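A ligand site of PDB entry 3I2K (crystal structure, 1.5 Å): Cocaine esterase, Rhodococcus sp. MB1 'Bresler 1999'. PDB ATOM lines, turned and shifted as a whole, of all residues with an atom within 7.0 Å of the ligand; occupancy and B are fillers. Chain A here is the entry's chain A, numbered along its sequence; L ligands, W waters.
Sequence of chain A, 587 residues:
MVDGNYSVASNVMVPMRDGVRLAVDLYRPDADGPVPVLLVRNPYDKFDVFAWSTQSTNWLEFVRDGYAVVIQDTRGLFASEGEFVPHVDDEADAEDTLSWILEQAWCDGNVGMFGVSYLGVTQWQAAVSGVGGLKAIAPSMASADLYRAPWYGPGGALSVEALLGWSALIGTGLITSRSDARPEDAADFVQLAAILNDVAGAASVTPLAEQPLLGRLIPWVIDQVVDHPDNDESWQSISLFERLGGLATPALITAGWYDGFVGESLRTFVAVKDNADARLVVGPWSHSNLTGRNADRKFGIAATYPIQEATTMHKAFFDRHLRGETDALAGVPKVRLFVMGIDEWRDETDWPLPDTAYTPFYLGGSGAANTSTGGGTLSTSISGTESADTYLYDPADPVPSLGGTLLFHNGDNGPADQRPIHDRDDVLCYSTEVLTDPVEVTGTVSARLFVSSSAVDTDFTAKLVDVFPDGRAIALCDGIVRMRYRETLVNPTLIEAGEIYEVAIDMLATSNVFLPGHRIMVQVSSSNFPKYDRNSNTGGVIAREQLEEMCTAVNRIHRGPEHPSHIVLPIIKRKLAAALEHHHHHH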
ATOM      1  N   PRO A  43      16.478  18.336  11.245  1.00  0.00           N
ATOM      2  CA  PRO A  43      16.241  16.980  10.723  1.00  0.00           C
ATOM      3  C   PRO A  43      16.631  16.805   9.245  1.00  0.00           C
ATOM      4  O   PRO A  43      16.333  15.762   8.650  1.00  0.00           O
ATOM      5  CB  PRO A  43      14.731  16.833  10.878  1.00  0.00           C
ATOM      6  CG  PRO A  43      14.223  18.220  10.577  1.00  0.00           C
ATOM      7  CD  PRO A  43      15.275  19.184  11.117  1.00  0.00           C
ATOM      8  N   TYR A  44      17.283  17.804   8.671  1.00  0.00           N
ATOM      9  CA  TYR A  44      17.613  17.834   7.242  1.00  0.00           C
ATOM     10  C   TYR A  44      19.121  17.848   6.970  1.00  0.00           C
ATOM     11  O   TYR A  44      19.566  18.384   5.958  1.00  0.00           O
ATOM     12  CB  TYR A  44      16.974  19.046   6.569  1.00  0.00           C
ATOM     13  CG  TYR A  44      15.498  19.265   6.911  1.00  0.00           C
ATOM     14  CD1 TYR A  44      14.525  18.340   6.543  1.00  0.00           C
ATOM     15  CD2 TYR A  44      15.082  20.418   7.585  1.00  0.00           C
ATOM     16  CE1 TYR A  44      13.182  18.550   6.834  1.00  0.00           C
ATOM     17  CE2 TYR A  44      13.749  20.630   7.885  1.00  0.00           C
ATOM     18  CZ  TYR A  44      12.803  19.701   7.509  1.00  0.00           C
ATOM     19  OH  TYR A  44      11.478  19.906   7.813  1.00  0.00           O
ATOM     20  N   HIS A  87       8.687  15.071  16.264  1.00  0.00           N
ATOM     21  CA  HIS A  87       8.210  15.818  17.438  1.00  0.00           C
ATOM     22  C   HIS A  87       8.377  15.173  18.825  1.00  0.00           C
ATOM     23  O   HIS A  87       8.625  15.884  19.801  1.00  0.00           O
ATOM     24  CB  HIS A  87       6.746  16.240  17.311  1.00  0.00           C
ATOM     25  CG  HIS A  87       6.379  16.802  15.968  1.00  0.00           C
ATOM     26  ND1 HIS A  87       7.110  17.800  15.359  1.00  0.00           N
ATOM     27  CD2 HIS A  87       5.348  16.525  15.135  1.00  0.00           C
ATOM     28  CE1 HIS A  87       6.543  18.117  14.210  1.00  0.00           C
ATOM     29  NE2 HIS A  87       5.470  17.358  14.048  1.00  0.00           N
ATOM     30  N   VAL A 116      14.417  28.050  11.262  1.00  0.00           N
ATOM     31  CA  VAL A 116      13.154  28.137  10.552  1.00  0.00           C
ATOM     32  C   VAL A 116      12.433  26.778  10.476  1.00  0.00           C
ATOM     33  O   VAL A 116      13.076  25.736  10.374  1.00  0.00           O
ATOM     34  CB  VAL A 116      13.414  28.703   9.136  1.00  0.00           C
ATOM     35  CG1 VAL A 116      14.307  27.766   8.312  1.00  0.00           C
ATOM     36  CG2 VAL A 116      12.115  29.044   8.409  1.00  0.00           C
ATOM     37  N   SER A 117      11.103  26.815  10.499  1.00  0.00           N
ATOM     38  CA  SER A 117      10.276  25.636  10.239  1.00  0.00           C
ATOM     39  C   SER A 117      10.532  24.594  11.338  1.00  0.00           C
ATOM     40  O   SER A 117      10.307  24.887  12.497  1.00  0.00           O
ATOM     41  CB  SER A 117      10.544  25.119   8.808  1.00  0.00           C
ATOM     42  OG  SER A 117       9.518  24.273   8.328  1.00  0.00           O
ATOM     43  N   TYR A 118      11.013  23.386  11.025  1.00  0.00           N
ATOM     44  CA  TYR A 118      11.207  22.380  12.081  1.00  0.00           C
ATOM     45  C   TYR A 118      12.315  22.877  13.041  1.00  0.00           C
ATOM     46  O   TYR A 118      12.305  22.567  14.227  1.00  0.00           O
ATOM     47  CB  TYR A 118      11.596  21.043  11.452  1.00  0.00           C
ATOM     48  CG  TYR A 118      11.402  19.809  12.314  1.00  0.00           C
ATOM     49  CD1 TYR A 118      12.322  19.452  13.297  1.00  0.00           C
ATOM     50  CD2 TYR A 118      10.330  18.955  12.101  1.00  0.00           C
ATOM     51  CE1 TYR A 118      12.163  18.291  14.046  1.00  0.00           C
ATOM     52  CE2 TYR A 118      10.150  17.802  12.851  1.00  0.00           C
ATOM     53  CZ  TYR A 118      11.078  17.482  13.819  1.00  0.00           C
ATOM     54  OH  TYR A 118      10.912  16.327  14.565  1.00  0.00           O
ATOM     55  N   LEU A 119      13.245  23.666  12.496  1.00  0.00           N
ATOM     56  CA  LEU A 119      14.318  24.287  13.285  1.00  0.00           C
ATOM     57  C   LEU A 119      13.768  25.425  14.164  1.00  0.00           C
ATOM     58  O   LEU A 119      14.493  25.946  15.006  1.00  0.00           O
ATOM     59  CB  LEU A 119      15.408  24.851  12.368  1.00  0.00           C
ATOM     60  CG  LEU A 119      16.306  23.885  11.574  1.00  0.00           C
ATOM     61  CD1 LEU A 119      15.496  22.957  10.663  1.00  0.00           C
ATOM     62  CD2 LEU A 119      17.309  24.679  10.754  1.00  0.00           C
ATOM     63  N   GLY A 120      12.513  25.818  13.925  1.00  0.00           N
ATOM     64  CA  GLY A 120      11.753  26.750  14.771  1.00  0.00           C
ATOM     65  C   GLY A 120      10.870  26.047  15.796  1.00  0.00           C
ATOM     66  O   GLY A 120      10.836  26.443  16.972  1.00  0.00           O
ATOM     67  N   VAL A 121      10.136  25.028  15.376  1.00  0.00           N
ATOM     68  CA  VAL A 121       9.287  24.253  16.277  1.00  0.00           C
ATOM     69  C   VAL A 121      10.122  23.704  17.436  1.00  0.00           C
ATOM     70  O   VAL A 121       9.707  23.751  18.598  1.00  0.00           O
ATOM     71  CB  VAL A 121       8.603  23.073  15.527  1.00  0.00           C
ATOM     72  CG1 VAL A 121       7.909  22.125  16.503  1.00  0.00           C
ATOM     73  CG2 VAL A 121       7.615  23.596  14.468  1.00  0.00           C
ATOM     74  N   MET A 141       8.826  30.996  11.087  1.00  0.00           N
ATOM     75  CA  MET A 141       7.866  30.187  10.316  1.00  0.00           C
ATOM     76  C   MET A 141       7.589  28.858  11.071  1.00  0.00           C
ATOM     77  O   MET A 141       7.741  27.776  10.501  1.00  0.00           O
ATOM     78  CB  MET A 141       8.356  30.050   8.827  1.00  0.00           C
ATOM     79  CG  MET A 141       8.533  31.423   8.210  1.00  0.00           C
ATOM     80  SD  MET A 141       9.191  31.367   6.553  1.00  0.00           S
ATOM     81  CE  MET A 141      10.364  32.720   6.646  1.00  0.00           C
ATOM     82  N   LEU A 146       1.182  21.631  17.099  1.00  0.00           N
ATOM     83  CA  LEU A 146       1.412  20.937  15.822  1.00  0.00           C
ATOM     84  C   LEU A 146       0.101  20.512  15.142  1.00  0.00           C
ATOM     85  O   LEU A 146       0.064  20.359  13.915  1.00  0.00           O
ATOM     86  CB  LEU A 146       2.346  19.738  16.013  1.00  0.00           C
ATOM     87  CG  LEU A 146       3.827  20.074  16.194  1.00  0.00           C
ATOM     88  CD1 LEU A 146       4.379  20.990  15.083  1.00  0.00           C
ATOM     89  CD2 LEU A 146       4.106  20.643  17.581  1.00  0.00           C
ATOM     90  N   ALA A 149      -0.959  23.900  13.479  1.00  0.00           N
ATOM     91  CA  ALA A 149      -0.099  24.052  12.313  1.00  0.00           C
ATOM     92  C   ALA A 149       1.155  23.205  12.512  1.00  0.00           C
ATOM     93  O   ALA A 149       1.798  23.307  13.548  1.00  0.00           O
ATOM     94  CB  ALA A 149       0.302  25.527  12.091  1.00  0.00           C
ATOM     95  N   PRO A 150       1.551  22.407  11.511  1.00  0.00           N
ATOM     96  CA  PRO A 150       1.062  22.405  10.150  1.00  0.00           C
ATOM     97  C   PRO A 150       0.113  21.271   9.785  1.00  0.00           C
ATOM     98  O   PRO A 150      -0.306  21.209   8.632  1.00  0.00           O
ATOM     99  CB  PRO A 150       2.356  22.245   9.353  1.00  0.00           C
ATOM    100  CG  PRO A 150       3.151  21.292  10.199  1.00  0.00           C
ATOM    101  CD  PRO A 150       2.795  21.607  11.629  1.00  0.00           C
ATOM    102  N   TRP A 151      -0.222  20.370  10.716  1.00  0.00           N
ATOM    103  CA  TRP A 151      -0.836  19.119  10.280  1.00  0.00           C
ATOM    104  C   TRP A 151      -2.348  19.152  10.124  1.00  0.00           C
ATOM    105  O   TRP A 151      -2.862  18.530   9.189  1.00  0.00           O
ATOM    106  CB  TRP A 151      -0.381  17.950  11.164  1.00  0.00           C
ATOM    107  CG  TRP A 151       1.109  17.839  11.260  1.00  0.00           C
ATOM    108  CD1 TRP A 151       1.823  17.767  12.412  1.00  0.00           C
ATOM    109  CD2 TRP A 151       2.078  17.857  10.194  1.00  0.00           C
ATOM    110  NE1 TRP A 151       3.157  17.710  12.142  1.00  0.00           N
ATOM    111  CE2 TRP A 151       3.349  17.756  10.790  1.00  0.00           C
ATOM    112  CE3 TRP A 151       1.991  17.931   8.798  1.00  0.00           C
ATOM    113  CZ2 TRP A 151       4.525  17.749  10.051  1.00  0.00           C
ATOM    114  CZ3 TRP A 151       3.169  17.914   8.069  1.00  0.00           C
ATOM    115  CH2 TRP A 151       4.419  17.831   8.686  1.00  0.00           C
ATOM    116  N   ALA A 162       0.339  19.194   2.983  1.00  0.00           N
ATOM    117  CA  ALA A 162       1.496  19.409   3.843  1.00  0.00           C
ATOM    118  C   ALA A 162       2.033  18.079   4.381  1.00  0.00           C
ATOM    119  O   ALA A 162       3.236  17.827   4.360  1.00  0.00           O
ATOM    120  CB  ALA A 162       1.130  20.330   5.007  1.00  0.00           C
ATOM    121  N   LEU A 163       1.126  17.241   4.876  1.00  0.00           N
ATOM    122  CA  LEU A 163       1.514  15.948   5.425  1.00  0.00           C
ATOM    123  C   LEU A 163       2.210  15.046   4.402  1.00  0.00           C
ATOM    124  O   LEU A 163       3.274  14.491   4.676  1.00  0.00           O
ATOM    125  CB  LEU A 163       0.292  15.219   5.959  1.00  0.00           C
ATOM    126  CG  LEU A 163       0.590  13.846   6.546  1.00  0.00           C
ATOM    127  CD1 LEU A 163       1.537  13.998   7.746  1.00  0.00           C
ATOM    128  CD2 LEU A 163      -0.683  13.155   6.919  1.00  0.00           C
ATOM    129  N   GLY A 165       3.468  15.776   1.364  1.00  0.00           N
ATOM    130  CA  GLY A 165       4.676  16.373   0.843  1.00  0.00           C
ATOM    131  C   GLY A 165       5.843  16.262   1.813  1.00  0.00           C
ATOM    132  O   GLY A 165       6.954  15.843   1.440  1.00  0.00           O
ATOM    133  N   TRP A 166       5.611  16.613   3.068  1.00  0.00           N
ATOM    134  CA  TRP A 166       6.701  16.591   4.037  1.00  0.00           C
ATOM    135  C   TRP A 166       7.157  15.170   4.305  1.00  0.00           C
ATOM    136  O   TRP A 166       8.348  14.908   4.394  1.00  0.00           O
ATOM    137  CB  TRP A 166       6.281  17.256   5.340  1.00  0.00           C
ATOM    138  CG  TRP A 166       7.435  17.425   6.284  1.00  0.00           C
ATOM    139  CD1 TRP A 166       8.461  18.302   6.162  1.00  0.00           C
ATOM    140  CD2 TRP A 166       7.669  16.688   7.492  1.00  0.00           C
ATOM    141  NE1 TRP A 166       9.323  18.168   7.220  1.00  0.00           N
ATOM    142  CE2 TRP A 166       8.852  17.197   8.057  1.00  0.00           C
ATOM    143  CE3 TRP A 166       6.988  15.664   8.155  1.00  0.00           C
ATOM    144  CZ2 TRP A 166       9.387  16.709   9.255  1.00  0.00           C
ATOM    145  CZ3 TRP A 166       7.523  15.175   9.353  1.00  0.00           C
ATOM    146  CH2 TRP A 166       8.701  15.714   9.887  1.00  0.00           C
ATOM    147  N   LEU A 169       9.395  14.098   1.642  1.00  0.00           N
ATOM    148  CA  LEU A 169      10.698  14.756   1.796  1.00  0.00           C
ATOM    149  C   LEU A 169      11.534  14.066   2.877  1.00  0.00           C
ATOM    150  O   LEU A 169      12.708  13.760   2.662  1.00  0.00           O
ATOM    151  CB  LEU A 169      10.495  16.241   2.110  1.00  0.00           C
ATOM    152  CG  LEU A 169      11.719  17.080   2.412  1.00  0.00           C
ATOM    153  CD1 LEU A 169      12.633  17.139   1.198  1.00  0.00           C
ATOM    154  CD2 LEU A 169      11.297  18.484   2.854  1.00  0.00           C
ATOM    155  N   PHE A 261       2.379  28.286   8.552  1.00  0.00           N
ATOM    156  CA  PHE A 261       2.432  28.504   9.997  1.00  0.00           C
ATOM    157  C   PHE A 261       1.944  29.865  10.487  1.00  0.00           C
ATOM    158  O   PHE A 261       2.004  30.108  11.698  1.00  0.00           O
ATOM    159  CB  PHE A 261       3.860  28.326  10.482  1.00  0.00           C
ATOM    160  CG  PHE A 261       4.365  26.916  10.416  1.00  0.00           C
ATOM    161  CD1 PHE A 261       5.012  26.454   9.299  1.00  0.00           C
ATOM    162  CD2 PHE A 261       4.235  26.088  11.500  1.00  0.00           C
ATOM    163  CE1 PHE A 261       5.496  25.153   9.262  1.00  0.00           C
ATOM    164  CE2 PHE A 261       4.702  24.803  11.470  1.00  0.00           C
ATOM    165  CZ  PHE A 261       5.335  24.342  10.357  1.00  0.00           C
ATOM    166  N   HIS A 287       6.119  29.325   2.447  1.00  0.00           N
ATOM    167  CA  HIS A 287       7.167  28.555   3.110  1.00  0.00           C
ATOM    168  C   HIS A 287       8.378  28.312   2.227  1.00  0.00           C
ATOM    169  O   HIS A 287       9.520  28.278   2.712  1.00  0.00           O
ATOM    170  CB  HIS A 287       6.603  27.220   3.613  1.00  0.00           C
ATOM    171  CG  HIS A 287       7.237  26.720   4.872  1.00  0.00           C
ATOM    172  ND1 HIS A 287       7.104  27.377   6.068  1.00  0.00           N
ATOM    173  CD2 HIS A 287       7.957  25.605   5.131  1.00  0.00           C
ATOM    174  CE1 HIS A 287       7.745  26.705   7.014  1.00  0.00           C
ATOM    175  NE2 HIS A 287       8.268  25.620   6.465  1.00  0.00           N
ATOM    176  N   LEU A 407       1.829  24.469   1.278  1.00  0.00           N
ATOM    177  CA  LEU A 407       3.216  24.191   1.674  1.00  0.00           C
ATOM    178  C   LEU A 407       4.015  23.491   0.580  1.00  0.00           C
ATOM    179  O   LEU A 407       5.072  23.971   0.181  1.00  0.00           O
ATOM    180  CB  LEU A 407       3.238  23.384   2.979  1.00  0.00           C
ATOM    181  CG  LEU A 407       2.949  24.188   4.254  1.00  0.00           C
ATOM    182  CD1 LEU A 407       2.702  23.308   5.466  1.00  0.00           C
ATOM    183  CD2 LEU A 407       4.096  25.125   4.575  1.00  0.00           C
ATOM    184  N   PHE A 408       3.484  22.369   0.087  1.00  0.00           N
ATOM    185  CA  PHE A 408       4.181  21.489  -0.867  1.00  0.00           C
ATOM    186  C   PHE A 408       3.547  21.393  -2.244  1.00  0.00           C
ATOM    187  O   PHE A 408       4.248  21.257  -3.233  1.00  0.00           O
ATOM    188  CB  PHE A 408       4.336  20.086  -0.275  1.00  0.00           C
ATOM    189  CG  PHE A 408       5.409  19.998   0.744  1.00  0.00           C
ATOM    190  CD1 PHE A 408       6.710  19.672   0.367  1.00  0.00           C
ATOM    191  CD2 PHE A 408       5.146  20.243   2.069  1.00  0.00           C
ATOM    192  CE1 PHE A 408       7.712  19.609   1.312  1.00  0.00           C
ATOM    193  CE2 PHE A 408       6.158  20.208   3.010  1.00  0.00           C
ATOM    194  CZ  PHE A 408       7.425  19.891   2.639  1.00  0.00           C
HETATM  195  O1  LIG L   1      11.053  22.430   8.194  1.00  0.00           O
HETATM  196  C1  LIG L   1       9.647  22.806   8.202  1.00  0.00           C
HETATM  197  O2  LIG L   1       8.924  22.447   6.972  1.00  0.00           O
HETATM  198  O3  LIG L   1       8.946  22.135   9.295  1.00  0.00           O
HETATM  199  C2  LIG L   1       7.657  21.753   8.841  1.00  0.00           C
HETATM  200  C3  LIG L   1       7.237  20.481   9.567  1.00  0.00           C
HETATM  201  S1  LIG L   1       6.957  20.760  11.334  1.00  0.00           S
HETATM  202  C4  LIG L   1       7.808  21.631   7.335  1.00  0.00           C
HETATM  203  C5  LIG L   1       6.599  22.074   6.515  1.00  0.00           C
HETATM  204  S2  LIG L   1       5.120  21.040   6.740  1.00  0.00           S
HETATM  205  O   HOH W   1      12.346  23.689   6.152  1.00  0.00           O
HETATM  206  O   HOH W   2       9.959  21.622   4.652  1.00  0.00           O
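A carbon (C1) of the ligand is covalently linked to the side-chain hydroxyl (OG) of Ser 117 (1.5 Å).
The side-chain hydroxyl of Tyr 44 lies within hydrogen-bond range of an oxygen (O1) of the ligand, at 2.6 Å.
The backbone NH (N) of Tyr 118 lies within hydrogen-bond range of an oxygen (O3) of the ligand (3.0 Å).
A ring nitrogen (NE2) of His 287 is in hydrogen-bond range of an oxygen (O2) of the ligand (3.3 Å).
A ring nitrogen (NE2) of His 287 sits at hydrogen-bond distance from the side-chain hydroxyl (OG) of Ser 117 (2.6 Å).
O of Met 141 sits close to N of Ser 117 (3.5 Å).
The side-chain hydroxyl of Tyr 44 is in hydrogen-bond range of the indole nitrogen of Trp 166 (2.8 Å).
The side-chain hydroxyl of Tyr 118 sits at hydrogen-bond distance from the backbone NH of His 87 (3.1 Å).
NE2 of His 87 is in hydrogen-bond range of NE1 of Trp 151, 3.0 Å away.
N of Trp 151 lies within hydrogen-bond range of O of Leu 146 (3.2 Å).
CE1 of His 87 touches S1 of the ligand (3.9 Å).
Pro 150 touches the ligand.
CH2 of Trp 151 touches S2 of the ligand, at 3.8 Å.
Trp 166 touches the ligand.
CZ of Phe 261 touches C2 of the ligand, at 3.8 Å.
Leu 407 touches the ligand.
CE2 of Phe 408 touches S2 of the ligand (3.96 Å).
Hydrophobic or aromatic side chains within 4 Å of the ligand: Tyr 44, His 87, Tyr 118, Pro 150, Trp 151, Trp 166, Phe 261, His 287, Leu 407 and Phe 408.
11 residues have an atom within 4 Å of the ligand: Tyr 44, His 87, Ser 117, Tyr 118, Pro 150, Trp 151, Trp 166, Phe 261, His 287, Leu 407 and Phe 408.
The nearest printed residue that does not touch the ligand is Val 121 (4.3 Å).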
